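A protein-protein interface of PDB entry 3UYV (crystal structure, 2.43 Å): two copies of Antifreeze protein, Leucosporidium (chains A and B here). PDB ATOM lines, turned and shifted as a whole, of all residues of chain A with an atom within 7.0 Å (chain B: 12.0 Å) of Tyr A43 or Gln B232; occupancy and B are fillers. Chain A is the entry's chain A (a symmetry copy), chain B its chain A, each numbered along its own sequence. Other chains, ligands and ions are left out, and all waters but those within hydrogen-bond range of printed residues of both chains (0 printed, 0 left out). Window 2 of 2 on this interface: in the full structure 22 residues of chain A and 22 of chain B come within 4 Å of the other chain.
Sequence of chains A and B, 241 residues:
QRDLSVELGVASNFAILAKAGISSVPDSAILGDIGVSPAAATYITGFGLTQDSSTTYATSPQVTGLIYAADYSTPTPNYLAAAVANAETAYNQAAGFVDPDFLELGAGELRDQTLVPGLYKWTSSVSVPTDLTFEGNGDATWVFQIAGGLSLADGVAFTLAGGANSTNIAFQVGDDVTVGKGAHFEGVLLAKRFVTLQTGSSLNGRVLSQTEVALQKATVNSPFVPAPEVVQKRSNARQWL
The backbone NH (N) of Ala A40 lies within hydrogen-bond range of the backbone carbonyl oxygen (O) of Val B231.
The backbone NH of Val B231 is in hydrogen-bond range of the backbone carbonyl oxygen of Pro A38 (2.9 Å).
The backbone carbonyl oxygen (O) of Gln B232 sits close to the side-chain hydroxyl (OH) of Tyr A43 (3.4 Å).
The backbone NH (N) of Ala A39 sits at hydrogen-bond distance from the backbone carbonyl oxygen (O) of Lys A19 (3.2 Å).
The backbone carbonyl oxygen of Ala A39 is in hydrogen-bond range of the backbone NH of Ala A70 (3.2 Å).
O of Val A36 lies within hydrogen-bond range of N of Ala A70, 3.2 Å away.
The backbone NH of Ile A22 lies within hydrogen-bond range of the backbone carbonyl oxygen of Tyr A43, 3.1 Å away.
Glu B229 touches Pro A38 (O to CB, 3.2 Å).
O of Pro A38 touches CA of Val B230, 3.5 Å away.
CA of Ala A39 touches O of Val B231, 3.7 Å away.
CG2 of Thr A42 touches O of Gln B232, at 3.6 Å.
Tyr A43 touches Val B231 (CE2 to O, 3.4 Å).
Val B230 touches Ala A70 (CG2 to O, 3.6 Å).
No residue of chain B comes within 4 Å of Ala A20.
No residue of chain B comes within 4 Å of Gly A21.
No residue of chain B comes within 4 Å of Ile A22.
No residue of chain B comes within 4 Å of Ser A23.
No residue of chain B comes within 4 Å of Ala A41.
Of the printed residues of chain B, Thr A42 touches Gln B232 (3.6 Å).
No residue of chain B comes within 4 Å of Ile A44.
Of the printed residues of chain B, Ala A70 touches Val B230.
Asp A71 touches none of the printed residues of chain B.
Of the printed residues of chain A, Val B231 touches Pro A38 (2.9 Å), Ala A39 (3.7 Å), Ala A40 (3.1 Å) and Tyr A43 (3.4 Å).
Of chain A, only Thr A42 and Tyr A43 come within 4 Å of Gln B232.
The nearest residue of chain B that does not touch Tyr A43 is Val B230 (7.5 Å).
The nearest printed residue of chain A that does not touch Glu B229 is Ala A39 (6.1 Å).
Of the 6 printed residues of chain B, 4 touch a printed residue of chain A.
Hydrophobic or aromatic side chains of chain B within 4 Å of the printed part of chain A: Val B230.
Hydrophobic or aromatic side chains of chain A that line the printed part of chain B: Pro A38, Ala A40 and Tyr A43.
No position is printed for both chains.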
ATOM      1  N   LYS A  19       4.224  -3.228  13.916  1.00  0.00           N
ATOM      2  CA  LYS A  19       2.794  -3.309  13.636  1.00  0.00           C
ATOM      3  C   LYS A  19       2.151  -1.962  13.472  1.00  0.00           C
ATOM      4  O   LYS A  19       1.276  -1.786  12.591  1.00  0.00           O
ATOM      5  CB  LYS A  19       2.079  -4.172  14.669  1.00  0.00           C
ATOM      6  CG  LYS A  19       2.320  -5.645  14.376  1.00  0.00           C
ATOM      7  CD  LYS A  19       1.660  -6.582  15.383  1.00  0.00           C
ATOM      8  CE  LYS A  19       0.205  -6.938  15.028  1.00  0.00           C
ATOM      9  NZ  LYS A  19      -0.253  -7.968  16.022  1.00  0.00           N
ATOM     10  N   ALA A  20       2.581  -0.982  14.279  1.00  0.00           N
ATOM     11  CA  ALA A  20       1.848   0.285  14.344  1.00  0.00           C
ATOM     12  C   ALA A  20       2.587   1.448  13.739  1.00  0.00           C
ATOM     13  O   ALA A  20       1.944   2.401  13.332  1.00  0.00           O
ATOM     14  CB  ALA A  20       1.422   0.604  15.755  1.00  0.00           C
ATOM     15  N   GLY A  21       3.924   1.418  13.696  1.00  0.00           N
ATOM     16  CA  GLY A  21       4.637   2.528  13.066  1.00  0.00           C
ATOM     17  C   GLY A  21       6.123   2.448  13.237  1.00  0.00           C
ATOM     18  O   GLY A  21       6.623   1.842  14.185  1.00  0.00           O
ATOM     19  N   ILE A  22       6.843   3.098  12.336  1.00  0.00           N
ATOM     20  CA  ILE A  22       8.290   3.310  12.480  1.00  0.00           C
ATOM     21  C   ILE A  22       8.592   4.812  12.271  1.00  0.00           C
ATOM     22  O   ILE A  22       8.089   5.428  11.302  1.00  0.00           O
ATOM     23  CB  ILE A  22       9.109   2.481  11.454  1.00  0.00           C
ATOM     24  CG1 ILE A  22       8.817   0.979  11.582  1.00  0.00           C
ATOM     25  CG2 ILE A  22      10.638   2.672  11.658  1.00  0.00           C
ATOM     26  CD1 ILE A  22       9.393   0.179  10.384  1.00  0.00           C
ATOM     27  N   SER A  23       9.408   5.393  13.153  1.00  0.00           N
ATOM     28  CA  SER A  23       9.819   6.810  13.029  1.00  0.00           C
ATOM     29  C   SER A  23      11.324   6.992  13.071  1.00  0.00           C
ATOM     30  O   SER A  23      12.039   6.162  13.615  1.00  0.00           O
ATOM     31  CB  SER A  23       9.192   7.672  14.128  1.00  0.00           C
ATOM     32  OG  SER A  23       9.277   7.073  15.408  1.00  0.00           O
ATOM     33  N   VAL A  36       5.887  -1.965   7.820  1.00  0.00           N
ATOM     34  CA  VAL A  36       4.821  -1.872   8.824  1.00  0.00           C
ATOM     35  C   VAL A  36       3.592  -2.604   8.283  1.00  0.00           C
ATOM     36  O   VAL A  36       3.265  -2.480   7.102  1.00  0.00           O
ATOM     37  CB  VAL A  36       4.506  -0.391   9.276  1.00  0.00           C
ATOM     38  CG1 VAL A  36       5.760   0.290   9.820  1.00  0.00           C
ATOM     39  CG2 VAL A  36       3.935   0.441   8.151  1.00  0.00           C
ATOM     40  N   PRO A  38      -0.247  -4.248  10.403  1.00  0.00           N
ATOM     41  CA  PRO A  38      -1.242  -3.734   9.429  1.00  0.00           C
ATOM     42  C   PRO A  38      -1.233  -2.226   9.154  1.00  0.00           C
ATOM     43  O   PRO A  38      -1.995  -1.780   8.300  1.00  0.00           O
ATOM     44  CB  PRO A  38      -2.605  -4.112  10.052  1.00  0.00           C
ATOM     45  CG  PRO A  38      -2.369  -4.247  11.488  1.00  0.00           C
ATOM     46  CD  PRO A  38      -0.899  -4.710  11.642  1.00  0.00           C
ATOM     47  N   ALA A  39      -0.417  -1.440   9.851  1.00  0.00           N
ATOM     48  CA  ALA A  39      -0.271  -0.005   9.518  1.00  0.00           C
ATOM     49  C   ALA A  39       0.048   0.275   8.057  1.00  0.00           C
ATOM     50  O   ALA A  39       0.790  -0.478   7.413  1.00  0.00           O
ATOM     51  CB  ALA A  39       0.781   0.652  10.410  1.00  0.00           C
ATOM     52  N   ALA A  40      -0.542   1.363   7.546  1.00  0.00           N
ATOM     53  CA  ALA A  40      -0.272   1.914   6.226  1.00  0.00           C
ATOM     54  C   ALA A  40       0.976   2.812   6.250  1.00  0.00           C
ATOM     55  O   ALA A  40       1.511   3.101   7.318  1.00  0.00           O
ATOM     56  CB  ALA A  40      -1.473   2.731   5.787  1.00  0.00           C
ATOM     57  N   ALA A  41       1.392   3.289   5.076  1.00  0.00           N
ATOM     58  CA  ALA A  41       2.619   4.062   4.902  1.00  0.00           C
ATOM     59  C   ALA A  41       2.722   5.405   5.632  1.00  0.00           C
ATOM     60  O   ALA A  41       3.820   5.868   5.919  1.00  0.00           O
ATOM     61  CB  ALA A  41       2.945   4.234   3.409  1.00  0.00           C
ATOM     62  N   THR A  42       1.581   6.023   5.922  1.00  0.00           N
ATOM     63  CA  THR A  42       1.485   7.308   6.650  1.00  0.00           C
ATOM     64  C   THR A  42       2.156   7.230   8.041  1.00  0.00           C
ATOM     65  O   THR A  42       2.630   8.248   8.564  1.00  0.00           O
ATOM     66  CB  THR A  42      -0.030   7.742   6.779  1.00  0.00           C
ATOM     67  OG1 THR A  42      -0.168   8.887   7.648  1.00  0.00           O
ATOM     68  CG2 THR A  42      -0.841   6.626   7.336  1.00  0.00           C
ATOM     69  N   TYR A  43       2.211   6.027   8.611  1.00  0.00           N
ATOM     70  CA  TYR A  43       2.841   5.753   9.897  1.00  0.00           C
ATOM     71  C   TYR A  43       4.339   5.401   9.857  1.00  0.00           C
ATOM     72  O   TYR A  43       4.905   5.004  10.876  1.00  0.00           O
ATOM     73  CB  TYR A  43       2.092   4.612  10.563  1.00  0.00           C
ATOM     74  CG  TYR A  43       0.649   4.918  10.812  1.00  0.00           C
ATOM     75  CD1 TYR A  43       0.271   5.738  11.895  1.00  0.00           C
ATOM     76  CD2 TYR A  43      -0.344   4.407   9.979  1.00  0.00           C
ATOM     77  CE1 TYR A  43      -1.085   6.065  12.127  1.00  0.00           C
ATOM     78  CE2 TYR A  43      -1.674   4.698  10.199  1.00  0.00           C
ATOM     79  CZ  TYR A  43      -2.050   5.539  11.273  1.00  0.00           C
ATOM     80  OH  TYR A  43      -3.395   5.823  11.502  1.00  0.00           O
ATOM     81  N   ILE A  44       4.977   5.524   8.694  1.00  0.00           N
ATOM     82  CA  ILE A  44       6.442   5.510   8.591  1.00  0.00           C
ATOM     83  C   ILE A  44       6.849   6.975   8.441  1.00  0.00           C
ATOM     84  O   ILE A  44       6.704   7.531   7.359  1.00  0.00           O
ATOM     85  CB  ILE A  44       6.943   4.680   7.347  1.00  0.00           C
ATOM     86  CG1 ILE A  44       6.445   3.232   7.413  1.00  0.00           C
ATOM     87  CG2 ILE A  44       8.462   4.672   7.220  1.00  0.00           C
ATOM     88  CD1 ILE A  44       6.643   2.433   6.100  1.00  0.00           C
ATOM     89  N   THR A  45       7.368   7.588   9.510  1.00  0.00           N
ATOM     90  CA  THR A  45       7.650   9.054   9.563  1.00  0.00           C
ATOM     91  C   THR A  45       9.142   9.439   9.706  1.00  0.00           C
ATOM     92  O   THR A  45       9.937   8.786  10.443  1.00  0.00           O
ATOM     93  CB  THR A  45       6.887   9.725  10.726  1.00  0.00           C
ATOM     94  OG1 THR A  45       7.120   9.002  11.946  1.00  0.00           O
ATOM     95  CG2 THR A  45       5.383   9.762  10.440  1.00  0.00           C
ATOM     96  N   ALA A  70       1.481  -1.731   4.604  1.00  0.00           N
ATOM     97  CA  ALA A  70       0.355  -2.655   4.392  1.00  0.00           C
ATOM     98  C   ALA A  70      -0.644  -2.208   3.332  1.00  0.00           C
ATOM     99  O   ALA A  70      -1.525  -2.974   2.956  1.00  0.00           O
ATOM    100  CB  ALA A  70      -0.379  -2.937   5.720  1.00  0.00           C
ATOM    101  N   ASP A  71      -0.527  -0.971   2.879  1.00  0.00           N
ATOM    102  CA  ASP A  71      -1.461  -0.384   1.906  1.00  0.00           C
ATOM    103  C   ASP A  71      -0.782  -0.210   0.565  1.00  0.00           C
ATOM    104  O   ASP A  71      -1.271   0.493  -0.295  1.00  0.00           O
ATOM    105  CB  ASP A  71      -2.009   0.971   2.436  1.00  0.00           C
ATOM    106  CG  ASP A  71      -0.941   2.082   2.505  1.00  0.00           C
ATOM    107  OD1 ASP A  71       0.250   1.816   2.841  1.00  0.00           O
ATOM    108  OD2 ASP A  71      -1.299   3.251   2.228  1.00  0.00           O
ATOM    109  N   GLU A 212       5.358   0.000  18.155  1.00  0.00           N
ATOM    110  CA  GLU A 212       6.019   1.061  17.417  1.00  0.00           C
ATOM    111  C   GLU A 212       7.532   1.099  17.624  1.00  0.00           C
ATOM    112  O   GLU A 212       8.047   0.752  18.709  1.00  0.00           O
ATOM    113  CB  GLU A 212       5.376   2.374  17.823  1.00  0.00           C
ATOM    114  CG  GLU A 212       5.170   3.348  16.701  1.00  0.00           C
ATOM    115  CD  GLU A 212       4.120   4.429  17.002  1.00  0.00           C
ATOM    116  OE1 GLU A 212       3.238   4.245  17.894  1.00  0.00           O
ATOM    117  OE2 GLU A 212       4.198   5.468  16.298  1.00  0.00           O
ATOM    118  N   VAL A 213       8.250   1.465  16.554  1.00  0.00           N
ATOM    119  CA  VAL A 213       9.714   1.573  16.591  1.00  0.00           C
ATOM    120  C   VAL A 213      10.190   2.994  16.344  1.00  0.00           C
ATOM    121  O   VAL A 213       9.883   3.580  15.268  1.00  0.00           O
ATOM    122  CB  VAL A 213      10.390   0.612  15.593  1.00  0.00           C
ATOM    123  CG1 VAL A 213      11.892   0.907  15.477  1.00  0.00           C
ATOM    124  CG2 VAL A 213      10.224  -0.791  16.054  1.00  0.00           C
ATOM    125  N   ALA B 227      -8.436 -11.388   3.760  1.00  0.00           N
ATOM    126  CA  ALA B 227      -7.877 -10.063   3.575  1.00  0.00           C
ATOM    127  C   ALA B 227      -7.164  -9.609   4.887  1.00  0.00           C
ATOM    128  O   ALA B 227      -7.828  -9.474   5.938  1.00  0.00           O
ATOM    129  CB  ALA B 227      -8.983  -9.086   3.187  1.00  0.00           C
ATOM    130  N   PRO B 228      -5.812  -9.424   4.838  1.00  0.00           N
ATOM    131  CA  PRO B 228      -5.079  -8.837   5.977  1.00  0.00           C
ATOM    132  C   PRO B 228      -5.617  -7.423   6.199  1.00  0.00           C
ATOM    133  O   PRO B 228      -5.644  -6.633   5.242  1.00  0.00           O
ATOM    134  CB  PRO B 228      -3.625  -8.783   5.471  1.00  0.00           C
ATOM    135  CG  PRO B 228      -3.743  -8.796   3.935  1.00  0.00           C
ATOM    136  CD  PRO B 228      -4.923  -9.687   3.675  1.00  0.00           C
ATOM    137  N   GLU B 229      -6.072  -7.112   7.416  1.00  0.00           N
ATOM    138  CA  GLU B 229      -6.907  -5.911   7.602  1.00  0.00           C
ATOM    139  C   GLU B 229      -6.113  -4.655   7.980  1.00  0.00           C
ATOM    140  O   GLU B 229      -5.643  -4.539   9.113  1.00  0.00           O
ATOM    141  CB  GLU B 229      -8.124  -6.163   8.550  1.00  0.00           C
ATOM    142  CG  GLU B 229      -7.877  -7.085   9.810  1.00  0.00           C
ATOM    143  CD  GLU B 229      -9.045  -7.081  10.848  1.00  0.00           C
ATOM    144  OE1 GLU B 229     -10.231  -7.316  10.462  1.00  0.00           O
ATOM    145  OE2 GLU B 229      -8.765  -6.851  12.061  1.00  0.00           O
ATOM    146  N   VAL B 230      -6.030  -3.728   7.016  1.00  0.00           N
ATOM    147  CA  VAL B 230      -5.235  -2.477   7.059  1.00  0.00           C
ATOM    148  C   VAL B 230      -5.683  -1.402   8.093  1.00  0.00           C
ATOM    149  O   VAL B 230      -6.880  -1.160   8.303  1.00  0.00           O
ATOM    150  CB  VAL B 230      -5.136  -1.834   5.618  1.00  0.00           C
ATOM    151  CG1 VAL B 230      -4.205  -0.600   5.578  1.00  0.00           C
ATOM    152  CG2 VAL B 230      -4.684  -2.871   4.582  1.00  0.00           C
ATOM    153  N   VAL B 231      -4.697  -0.777   8.739  1.00  0.00           N
ATOM    154  CA  VAL B 231      -4.927   0.357   9.638  1.00  0.00           C
ATOM    155  C   VAL B 231      -4.477   1.645   8.909  1.00  0.00           C
ATOM    156  O   VAL B 231      -3.291   1.976   8.834  1.00  0.00           O
ATOM    157  CB  VAL B 231      -4.253   0.131  11.064  1.00  0.00           C
ATOM    158  CG1 VAL B 231      -4.277   1.405  11.941  1.00  0.00           C
ATOM    159  CG2 VAL B 231      -4.918  -1.040  11.812  1.00  0.00           C
ATOM    160  N   GLN B 232      -5.449   2.329   8.313  1.00  0.00           N
ATOM    161  CA  GLN B 232      -5.213   3.569   7.577  1.00  0.00           C
ATOM    162  C   GLN B 232      -4.899   4.677   8.584  1.00  0.00           C
ATOM    163  O   GLN B 232      -4.205   5.628   8.253  1.00  0.00           O
ATOM    164  CB  GLN B 232      -6.449   3.950   6.729  1.00  0.00           C
ATOM    165  CG  GLN B 232      -6.833   2.994   5.553  1.00  0.00           C
ATOM    166  CD  GLN B 232      -5.953   3.137   4.266  1.00  0.00           C
ATOM    167  OE1 GLN B 232      -5.167   4.084   4.114  1.00  0.00           O
ATOM    168  NE2 GLN B 232      -6.101   2.177   3.343  1.00  0.00           N
